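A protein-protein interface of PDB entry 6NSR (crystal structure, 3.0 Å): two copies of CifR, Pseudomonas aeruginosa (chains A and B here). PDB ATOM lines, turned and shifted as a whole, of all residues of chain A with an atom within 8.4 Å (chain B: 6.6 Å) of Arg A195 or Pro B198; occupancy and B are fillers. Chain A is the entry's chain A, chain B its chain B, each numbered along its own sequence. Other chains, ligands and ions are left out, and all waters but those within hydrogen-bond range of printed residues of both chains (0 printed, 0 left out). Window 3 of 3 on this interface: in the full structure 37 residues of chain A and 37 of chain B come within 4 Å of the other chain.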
ATOM      1  N   ARG A  86       8.065  27.698 -24.011  1.00  0.00           N
ATOM      2  CA  ARG A  86       9.133  26.708 -24.099  1.00  0.00           C
ATOM      3  C   ARG A  86      10.453  27.285 -23.602  1.00  0.00           C
ATOM      4  O   ARG A  86      11.173  26.642 -22.828  1.00  0.00           O
ATOM      5  CB  ARG A  86       9.258  26.173 -25.526  1.00  0.00           C
ATOM      6  CG  ARG A  86      10.400  25.188 -25.709  1.00  0.00           C
ATOM      7  CD  ARG A  86      10.327  24.505 -27.061  1.00  0.00           C
ATOM      8  NE  ARG A  86      11.361  23.488 -27.212  1.00  0.00           N
ATOM      9  CZ  ARG A  86      11.412  22.615 -28.209  1.00  0.00           C
ATOM     10  NH1 ARG A  86      10.500  22.604 -29.167  1.00  0.00           N
ATOM     11  NH2 ARG A  86      12.404  21.728 -28.245  1.00  0.00           N
ATOM     12  N   LEU A  93      14.719  25.672 -16.060  1.00  0.00           N
ATOM     13  CA  LEU A  93      15.437  24.439 -15.750  1.00  0.00           C
ATOM     14  C   LEU A  93      16.944  24.656 -15.781  1.00  0.00           C
ATOM     15  O   LEU A  93      17.674  24.088 -14.961  1.00  0.00           O
ATOM     16  CB  LEU A  93      15.036  23.347 -16.738  1.00  0.00           C
ATOM     17  CG  LEU A  93      13.610  22.807 -16.653  1.00  0.00           C
ATOM     18  CD1 LEU A  93      13.341  21.838 -17.793  1.00  0.00           C
ATOM     19  CD2 LEU A  93      13.385  22.134 -15.320  1.00  0.00           C
ATOM     20  N   PHE A 165       4.975  16.962 -16.046  1.00  0.00           N
ATOM     21  CA  PHE A 165       6.198  16.352 -16.562  1.00  0.00           C
ATOM     22  C   PHE A 165       7.426  17.175 -16.196  1.00  0.00           C
ATOM     23  O   PHE A 165       8.423  16.638 -15.701  1.00  0.00           O
ATOM     24  CB  PHE A 165       6.107  16.175 -18.078  1.00  0.00           C
ATOM     25  CG  PHE A 165       7.428  15.869 -18.726  1.00  0.00           C
ATOM     26  CD1 PHE A 165       7.964  14.593 -18.669  1.00  0.00           C
ATOM     27  CD2 PHE A 165       8.139  16.860 -19.383  1.00  0.00           C
ATOM     28  CE1 PHE A 165       9.181  14.311 -19.258  1.00  0.00           C
ATOM     29  CE2 PHE A 165       9.358  16.585 -19.974  1.00  0.00           C
ATOM     30  CZ  PHE A 165       9.879  15.307 -19.911  1.00  0.00           C
ATOM     31  N   TYR A 166       7.371  18.489 -16.421  1.00  0.00           N
ATOM     32  CA  TYR A 166       8.541  19.314 -16.146  1.00  0.00           C
ATOM     33  C   TYR A 166       8.753  19.504 -14.650  1.00  0.00           C
ATOM     34  O   TYR A 166       9.890  19.701 -14.207  1.00  0.00           O
ATOM     35  CB  TYR A 166       8.463  20.635 -16.911  1.00  0.00           C
ATOM     36  CG  TYR A 166       8.829  20.473 -18.370  1.00  0.00           C
ATOM     37  CD1 TYR A 166      10.129  20.154 -18.747  1.00  0.00           C
ATOM     38  CD2 TYR A 166       7.872  20.608 -19.366  1.00  0.00           C
ATOM     39  CE1 TYR A 166      10.469  19.991 -20.079  1.00  0.00           C
ATOM     40  CE2 TYR A 166       8.202  20.447 -20.699  1.00  0.00           C
ATOM     41  CZ  TYR A 166       9.501  20.139 -21.051  1.00  0.00           C
ATOM     42  OH  TYR A 166       9.832  19.979 -22.377  1.00  0.00           O
ATOM     43  N   ALA A 188      22.666  18.659 -19.669  1.00  0.00           N
ATOM     44  CA  ALA A 188      22.315  17.734 -20.741  1.00  0.00           C
ATOM     45  C   ALA A 188      20.946  17.111 -20.501  1.00  0.00           C
ATOM     46  O   ALA A 188      20.159  16.941 -21.440  1.00  0.00           O
ATOM     47  CB  ALA A 188      23.386  16.654 -20.875  1.00  0.00           C
ATOM     48  N   VAL A 189      20.648  16.756 -19.249  1.00  0.00           N
ATOM     49  CA  VAL A 189      19.330  16.222 -18.915  1.00  0.00           C
ATOM     50  C   VAL A 189      18.245  17.256 -19.192  1.00  0.00           C
ATOM     51  O   VAL A 189      17.155  16.919 -19.671  1.00  0.00           O
ATOM     52  CB  VAL A 189      19.307  15.730 -17.455  1.00  0.00           C
ATOM     53  CG1 VAL A 189      17.885  15.424 -17.006  1.00  0.00           C
ATOM     54  CG2 VAL A 189      20.189  14.507 -17.303  1.00  0.00           C
ATOM     55  N   VAL A 190      18.527  18.530 -18.906  1.00  0.00           N
ATOM     56  CA  VAL A 190      17.546  19.585 -19.153  1.00  0.00           C
ATOM     57  C   VAL A 190      17.240  19.704 -20.640  1.00  0.00           C
ATOM     58  O   VAL A 190      16.075  19.799 -21.046  1.00  0.00           O
ATOM     59  CB  VAL A 190      18.028  20.919 -18.557  1.00  0.00           C
ATOM     60  CG1 VAL A 190      17.270  22.084 -19.175  1.00  0.00           C
ATOM     61  CG2 VAL A 190      17.859  20.909 -17.051  1.00  0.00           C
ATOM     62  N   GLU A 191      18.278  19.692 -21.478  1.00  0.00           N
ATOM     63  CA  GLU A 191      18.046  19.772 -22.918  1.00  0.00           C
ATOM     64  C   GLU A 191      17.317  18.537 -23.429  1.00  0.00           C
ATOM     65  O   GLU A 191      16.435  18.642 -24.291  1.00  0.00           O
ATOM     66  CB  GLU A 191      19.367  19.973 -23.660  1.00  0.00           C
ATOM     67  CG  GLU A 191      20.160  21.171 -23.177  1.00  0.00           C
ATOM     68  CD  GLU A 191      19.355  22.463 -23.225  1.00  0.00           C
ATOM     69  OE1 GLU A 191      18.653  22.696 -24.234  1.00  0.00           O
ATOM     70  OE2 GLU A 191      19.420  23.242 -22.250  1.00  0.00           O
ATOM     71  N   ARG A 192      17.673  17.360 -22.911  1.00  0.00           N
ATOM     72  CA  ARG A 192      16.958  16.139 -23.266  1.00  0.00           C
ATOM     73  C   ARG A 192      15.484  16.232 -22.891  1.00  0.00           C
ATOM     74  O   ARG A 192      14.614  15.791 -23.648  1.00  0.00           O
ATOM     75  CB  ARG A 192      17.616  14.939 -22.587  1.00  0.00           C
ATOM     76  CG  ARG A 192      16.887  13.625 -22.787  1.00  0.00           C
ATOM     77  CD  ARG A 192      16.865  13.234 -24.249  1.00  0.00           C
ATOM     78  NE  ARG A 192      18.206  13.212 -24.819  1.00  0.00           N
ATOM     79  CZ  ARG A 192      18.485  12.832 -26.059  1.00  0.00           C
ATOM     80  NH1 ARG A 192      17.538  12.421 -26.887  1.00  0.00           N
ATOM     81  NH2 ARG A 192      19.746  12.868 -26.479  1.00  0.00           N
ATOM     82  N   ALA A 193      15.184  16.810 -21.727  1.00  0.00           N
ATOM     83  CA  ALA A 193      13.794  16.960 -21.307  1.00  0.00           C
ATOM     84  C   ALA A 193      13.053  17.965 -22.180  1.00  0.00           C
ATOM     85  O   ALA A 193      11.862  17.792 -22.458  1.00  0.00           O
ATOM     86  CB  ALA A 193      13.728  17.364 -19.835  1.00  0.00           C
ATOM     87  N   LEU A 194      13.736  19.029 -22.605  1.00  0.00           N
ATOM     88  CA  LEU A 194      13.132  19.975 -23.538  1.00  0.00           C
ATOM     89  C   LEU A 194      12.810  19.324 -24.876  1.00  0.00           C
ATOM     90  O   LEU A 194      11.882  19.757 -25.568  1.00  0.00           O
ATOM     91  CB  LEU A 194      14.059  21.169 -23.744  1.00  0.00           C
ATOM     92  CG  LEU A 194      14.141  22.124 -22.558  1.00  0.00           C
ATOM     93  CD1 LEU A 194      15.362  23.015 -22.693  1.00  0.00           C
ATOM     94  CD2 LEU A 194      12.868  22.945 -22.452  1.00  0.00           C
ATOM     95  N   ARG A 195      13.577  18.303 -25.267  1.00  0.00           N
ATOM     96  CA  ARG A 195      13.282  17.573 -26.496  1.00  0.00           C
ATOM     97  C   ARG A 195      11.875  16.984 -26.485  1.00  0.00           C
ATOM     98  O   ARG A 195      11.281  16.776 -27.550  1.00  0.00           O
ATOM     99  CB  ARG A 195      14.336  16.486 -26.718  1.00  0.00           C
ATOM    100  CG  ARG A 195      14.149  15.665 -27.979  1.00  0.00           C
ATOM    101  CD  ARG A 195      15.315  14.719 -28.199  1.00  0.00           C
ATOM    102  NE  ARG A 195      14.991  13.682 -29.172  1.00  0.00           N
ATOM    103  CZ  ARG A 195      15.102  13.826 -30.485  1.00  0.00           C
ATOM    104  NH1 ARG A 195      15.511  14.964 -31.022  1.00  0.00           N
ATOM    105  NH2 ARG A 195      14.789  12.806 -31.280  1.00  0.00           N
ATOM    106  N   ALA A 196      11.314  16.733 -25.303  1.00  0.00           N
ATOM    107  CA  ALA A 196       9.975  16.164 -25.200  1.00  0.00           C
ATOM    108  C   ALA A 196       8.869  17.195 -25.385  1.00  0.00           C
ATOM    109  O   ALA A 196       7.689  16.832 -25.310  1.00  0.00           O
ATOM    110  CB  ALA A 196       9.801  15.454 -23.855  1.00  0.00           C
ATOM    111  N   TRP A 197       9.215  18.457 -25.630  1.00  0.00           N
ATOM    112  CA  TRP A 197       8.202  19.486 -25.803  1.00  0.00           C
ATOM    113  C   TRP A 197       7.429  19.245 -27.099  1.00  0.00           C
ATOM    114  O   TRP A 197       8.008  18.802 -28.097  1.00  0.00           O
ATOM    115  CB  TRP A 197       8.868  20.860 -25.858  1.00  0.00           C
ATOM    116  CG  TRP A 197       7.907  22.009 -25.848  1.00  0.00           C
ATOM    117  CD1 TRP A 197       7.238  22.528 -26.916  1.00  0.00           C
ATOM    118  CD2 TRP A 197       7.513  22.787 -24.710  1.00  0.00           C
ATOM    119  NE1 TRP A 197       6.447  23.579 -26.515  1.00  0.00           N
ATOM    120  CE2 TRP A 197       6.600  23.759 -25.166  1.00  0.00           C
ATOM    121  CE3 TRP A 197       7.842  22.756 -23.352  1.00  0.00           C
ATOM    122  CZ2 TRP A 197       6.012  24.689 -24.312  1.00  0.00           C
ATOM    123  CZ3 TRP A 197       7.259  23.681 -22.507  1.00  0.00           C
ATOM    124  CH2 TRP A 197       6.354  24.634 -22.989  1.00  0.00           C
ATOM    125  N   PRO A 198       6.114  19.509 -27.113  1.00  0.00           N
ATOM    126  CA  PRO A 198       5.308  19.377 -28.331  1.00  0.00           C
ATOM    127  C   PRO A 198       5.505  20.558 -29.275  1.00  0.00           C
ATOM    128  O   PRO A 198       6.400  20.506 -30.121  1.00  0.00           O
ATOM    129  CB  PRO A 198       3.877  19.370 -27.794  1.00  0.00           C
ATOM    130  CG  PRO A 198       3.953  20.184 -26.551  1.00  0.00           C
ATOM    131  CD  PRO A 198       5.290  19.864 -25.945  1.00  0.00           C
ATOM    132  OXT PRO A 198       4.783  21.552 -29.200  1.00  0.00           O
ATOM    133  N   ARG B  86      14.285   1.073 -26.126  1.00  0.00           N
ATOM    134  CA  ARG B  86      13.172   2.001 -25.949  1.00  0.00           C
ATOM    135  C   ARG B  86      12.009   1.324 -25.234  1.00  0.00           C
ATOM    136  O   ARG B  86      11.472   1.855 -24.255  1.00  0.00           O
ATOM    137  CB  ARG B  86      12.726   2.561 -27.299  1.00  0.00           C
ATOM    138  CG  ARG B  86      11.707   3.684 -27.186  1.00  0.00           C
ATOM    139  CD  ARG B  86      11.085   4.016 -28.530  1.00  0.00           C
ATOM    140  NE  ARG B  86      10.115   5.099 -28.424  1.00  0.00           N
ATOM    141  CZ  ARG B  86      10.338   6.344 -28.823  1.00  0.00           C
ATOM    142  NH1 ARG B  86      11.479   6.692 -29.397  1.00  0.00           N
ATOM    143  NH2 ARG B  86       9.390   7.261 -28.649  1.00  0.00           N
ATOM    144  N   ASP B 152      19.090  -1.171 -32.398  1.00  0.00           N
ATOM    145  CA  ASP B 152      17.933  -0.312 -32.185  1.00  0.00           C
ATOM    146  C   ASP B 152      18.299   1.037 -31.582  1.00  0.00           C
ATOM    147  O   ASP B 152      17.408   1.863 -31.357  1.00  0.00           O
ATOM    148  CB  ASP B 152      16.886  -1.021 -31.317  1.00  0.00           C
ATOM    149  CG  ASP B 152      17.432  -1.446 -29.968  1.00  0.00           C
ATOM    150  OD1 ASP B 152      17.545  -0.584 -29.071  1.00  0.00           O
ATOM    151  OD2 ASP B 152      17.746  -2.644 -29.803  1.00  0.00           O
ATOM    152  N   LEU B 153      19.580   1.275 -31.310  1.00  0.00           N
ATOM    153  CA  LEU B 153      20.063   2.550 -30.803  1.00  0.00           C
ATOM    154  C   LEU B 153      21.274   2.969 -31.622  1.00  0.00           C
ATOM    155  O   LEU B 153      22.127   2.137 -31.948  1.00  0.00           O
ATOM    156  CB  LEU B 153      20.463   2.441 -29.329  1.00  0.00           C
ATOM    157  CG  LEU B 153      19.620   3.233 -28.330  1.00  0.00           C
ATOM    158  CD1 LEU B 153      20.197   3.102 -26.932  1.00  0.00           C
ATOM    159  CD2 LEU B 153      19.524   4.693 -28.737  1.00  0.00           C
ATOM    160  N   ALA B 154      21.345   4.257 -31.951  1.00  0.00           N
ATOM    161  CA  ALA B 154      22.462   4.762 -32.736  1.00  0.00           C
ATOM    162  C   ALA B 154      23.771   4.597 -31.974  1.00  0.00           C
ATOM    163  O   ALA B 154      23.814   4.660 -30.743  1.00  0.00           O
ATOM    164  CB  ALA B 154      22.245   6.237 -33.075  1.00  0.00           C
ATOM    165  N   THR B 157      24.882   7.580 -29.856  1.00  0.00           N
ATOM    166  CA  THR B 157      23.908   8.029 -28.871  1.00  0.00           C
ATOM    167  C   THR B 157      24.610   8.398 -27.572  1.00  0.00           C
ATOM    168  O   THR B 157      25.443   7.640 -27.065  1.00  0.00           O
ATOM    169  CB  THR B 157      22.891   6.920 -28.601  1.00  0.00           C
ATOM    170  OG1 THR B 157      22.230   6.564 -29.822  1.00  0.00           O
ATOM    171  CG2 THR B 157      21.857   7.375 -27.582  1.00  0.00           C
ATOM    172  N   ASP B 158      24.274   9.567 -27.031  1.00  0.00           N
ATOM    173  CA  ASP B 158      24.809   9.989 -25.739  1.00  0.00           C
ATOM    174  C   ASP B 158      24.058   9.185 -24.688  1.00  0.00           C
ATOM    175  O   ASP B 158      22.978   9.566 -24.232  1.00  0.00           O
ATOM    176  CB  ASP B 158      24.627  11.489 -25.545  1.00  0.00           C
ATOM    177  CG  ASP B 158      25.378  12.018 -24.337  1.00  0.00           C
ATOM    178  OD1 ASP B 158      26.068  11.222 -23.665  1.00  0.00           O
ATOM    179  OD2 ASP B 158      25.286  13.234 -24.067  1.00  0.00           O
ATOM    180  N   LEU B 162      21.086  10.090 -21.690  1.00  0.00           N
ATOM    181  CA  LEU B 162      19.781   9.446 -21.775  1.00  0.00           C
ATOM    182  C   LEU B 162      19.476   8.657 -20.507  1.00  0.00           C
ATOM    183  O   LEU B 162      18.368   8.741 -19.963  1.00  0.00           O
ATOM    184  CB  LEU B 162      19.740   8.538 -23.005  1.00  0.00           C
ATOM    185  CG  LEU B 162      18.366   8.221 -23.589  1.00  0.00           C
ATOM    186  CD1 LEU B 162      17.668   9.498 -24.029  1.00  0.00           C
ATOM    187  CD2 LEU B 162      18.507   7.259 -24.752  1.00  0.00           C
ATOM    188  N   TYR B 166      16.367   9.519 -17.850  1.00  0.00           N
ATOM    189  CA  TYR B 166      15.286   8.633 -17.432  1.00  0.00           C
ATOM    190  C   TYR B 166      15.374   8.303 -15.949  1.00  0.00           C
ATOM    191  O   TYR B 166      14.346   8.066 -15.306  1.00  0.00           O
ATOM    192  CB  TYR B 166      15.243   7.385 -18.313  1.00  0.00           C
ATOM    193  CG  TYR B 166      14.610   7.660 -19.658  1.00  0.00           C
ATOM    194  CD1 TYR B 166      13.250   7.927 -19.763  1.00  0.00           C
ATOM    195  CD2 TYR B 166      15.374   7.693 -20.816  1.00  0.00           C
ATOM    196  CE1 TYR B 166      12.667   8.195 -20.987  1.00  0.00           C
ATOM    197  CE2 TYR B 166      14.800   7.961 -22.045  1.00  0.00           C
ATOM    198  CZ  TYR B 166      13.447   8.212 -22.125  1.00  0.00           C
ATOM    199  OH  TYR B 166      12.872   8.477 -23.347  1.00  0.00           O
ATOM    200  N   LEU B 194       9.088   9.561 -22.868  1.00  0.00           N
ATOM    201  CA  LEU B 194       9.529   8.752 -23.995  1.00  0.00           C
ATOM    202  C   LEU B 194       9.662   9.565 -25.274  1.00  0.00           C
ATOM    203  O   LEU B 194      10.373   9.140 -26.191  1.00  0.00           O
ATOM    204  CB  LEU B 194       8.560   7.592 -24.214  1.00  0.00           C
ATOM    205  CG  LEU B 194       8.578   6.519 -23.127  1.00  0.00           C
ATOM    206  CD1 LEU B 194       7.401   5.575 -23.292  1.00  0.00           C
ATOM    207  CD2 LEU B 194       9.894   5.759 -23.150  1.00  0.00           C
ATOM    208  N   ARG B 195       9.005  10.725 -25.358  1.00  0.00           N
ATOM    209  CA  ARG B 195       9.139  11.557 -26.546  1.00  0.00           C
ATOM    210  C   ARG B 195      10.545  12.127 -26.673  1.00  0.00           C
ATOM    211  O   ARG B 195      10.974  12.463 -27.784  1.00  0.00           O
ATOM    212  CB  ARG B 195       8.104  12.685 -26.516  1.00  0.00           C
ATOM    213  CG  ARG B 195       8.145  13.613 -27.724  1.00  0.00           C
ATOM    214  CD  ARG B 195       7.012  14.626 -27.691  1.00  0.00           C
ATOM    215  NE  ARG B 195       7.264  15.757 -28.576  1.00  0.00           N
ATOM    216  CZ  ARG B 195       7.107  15.730 -29.892  1.00  0.00           C
ATOM    217  NH1 ARG B 195       6.705  14.638 -30.521  1.00  0.00           N
ATOM    218  NH2 ARG B 195       7.357  16.830 -30.596  1.00  0.00           N
ATOM    219  N   ALA B 196      11.280  12.217 -25.564  1.00  0.00           N
ATOM    220  CA  ALA B 196      12.659  12.683 -25.592  1.00  0.00           C
ATOM    221  C   ALA B 196      13.617  11.652 -26.169  1.00  0.00           C
ATOM    222  O   ALA B 196      14.791  11.977 -26.381  1.00  0.00           O
ATOM    223  CB  ALA B 196      13.103  13.054 -24.179  1.00  0.00           C
ATOM    224  N   TRP B 197      13.149  10.436 -26.437  1.00  0.00           N
ATOM    225  CA  TRP B 197      14.033   9.395 -26.935  1.00  0.00           C
ATOM    226  C   TRP B 197      14.540   9.764 -28.328  1.00  0.00           C
ATOM    227  O   TRP B 197      13.775  10.274 -29.154  1.00  0.00           O
ATOM    228  CB  TRP B 197      13.281   8.069 -26.991  1.00  0.00           C
ATOM    229  CG  TRP B 197      14.149   6.885 -27.267  1.00  0.00           C
ATOM    230  CD1 TRP B 197      14.556   6.434 -28.488  1.00  0.00           C
ATOM    231  CD2 TRP B 197      14.713   5.991 -26.300  1.00  0.00           C
ATOM    232  NE1 TRP B 197      15.342   5.316 -28.340  1.00  0.00           N
ATOM    233  CE2 TRP B 197      15.452   5.023 -27.006  1.00  0.00           C
ATOM    234  CE3 TRP B 197      14.663   5.917 -24.905  1.00  0.00           C
ATOM    235  CZ2 TRP B 197      16.138   3.995 -26.367  1.00  0.00           C
ATOM    236  CZ3 TRP B 197      15.345   4.894 -24.270  1.00  0.00           C
ATOM    237  CH2 TRP B 197      16.073   3.947 -25.001  1.00  0.00           C
ATOM    238  N   PRO B 198      15.829   9.528 -28.620  1.00  0.00           N
ATOM    239  CA  PRO B 198      16.401   9.834 -29.935  1.00  0.00           C
ATOM    240  C   PRO B 198      15.925   8.870 -31.015  1.00  0.00           C
ATOM    241  O   PRO B 198      15.334   9.327 -31.995  1.00  0.00           O
ATOM    242  CB  PRO B 198      17.903   9.662 -29.707  1.00  0.00           C
ATOM    243  CG  PRO B 198      17.995   8.665 -28.609  1.00  0.00           C
ATOM    244  CD  PRO B 198      16.832   8.957 -27.705  1.00  0.00           C
ATOM    245  OXT PRO B 198      16.125   7.660 -30.912  1.00  0.00           O
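Leu B162 touches Arg A192 (CD1 to CD, 3.8 Å).
Pro B198 touches Arg A192 (CD to NH1, 3.6 Å).
Ala A196 touches Ala B196.
O of Ala B196 sits at hydrogen-bond distance from NH1 of Arg A192 (2.8 Å).
The guanidinium group (NE) of Arg A195 sits at hydrogen-bond distance from the backbone carbonyl oxygen (O) of Ala B196 (3.3 Å).
The guanidinium group (NH2) of Arg A195 sits at hydrogen-bond distance from the backbone carbonyl oxygen (O) of Trp B197, at 3.5 Å.
The chain-end carboxylate (O) of Pro B198 is in salt-bridge range of the guanidinium group (NH2) of Arg A195 (3.6 Å).
The guanidinium group of Arg B195 lies close to the backbone carbonyl oxygen of Ala A196 (3.5 Å).
The backbone carbonyl oxygen (O) of Trp A197 is in hydrogen-bond range of the guanidinium group (NE) of Arg B195 (3.2 Å).
The guanidinium group (NH2) of Arg B195 lies within salt-bridge range of the chain-end carboxylate (O) of Pro A198.
Leu A194 touches none of the printed residues of chain B.
Of chain B, only Ala B196, Trp B197 and Pro B198 come within 4 Å of Arg A195.
Leu B194 touches none of the printed residues of chain A.
Of the printed residues of chain A, Arg B195 touches Ala A196 (3.3 Å), Trp A197 (3.2 Å) and Pro A198 (3.8 Å).
Printed residues of chain A within 4 Å of Ala B196: Arg A192, Arg A195 and Ala A196.
Printed residues of chain A within 4 Å of Trp B197: Arg A195 (3.5 Å).
Of chain A, only Arg A192 (3.6 Å) and Arg A195 (3.6 Å) come within 4 Å of Pro B198.
The nearest residue of chain B that does not touch Arg A195 is Arg B195 (4.3 Å).
The nearest printed residue of chain A that does not touch Pro B198 is Ala A196 (9.1 Å).
Arg A195 touches Ala B196, and with the chains exchanged Ala A196 touches Arg B195.
Arg A195 touches Trp B197, and with the chains exchanged Trp A197 touches Arg B195.
Arg A195 touches Pro B198, and with the chains exchanged Pro A198 touches Arg B195.
Ala B196 touches its own counterpart, Ala A196.
Positions printed for both chains: 86, 166, 194, 195, 196, 197 and 198.
Along chain B the printed residues that touch a printed residue of chain A span positions 162 to 198.
Among the printed residues, no Asp or Glu carboxylate lies within 4 Å of a Lys or Arg side-chain nitrogen of the other chain.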
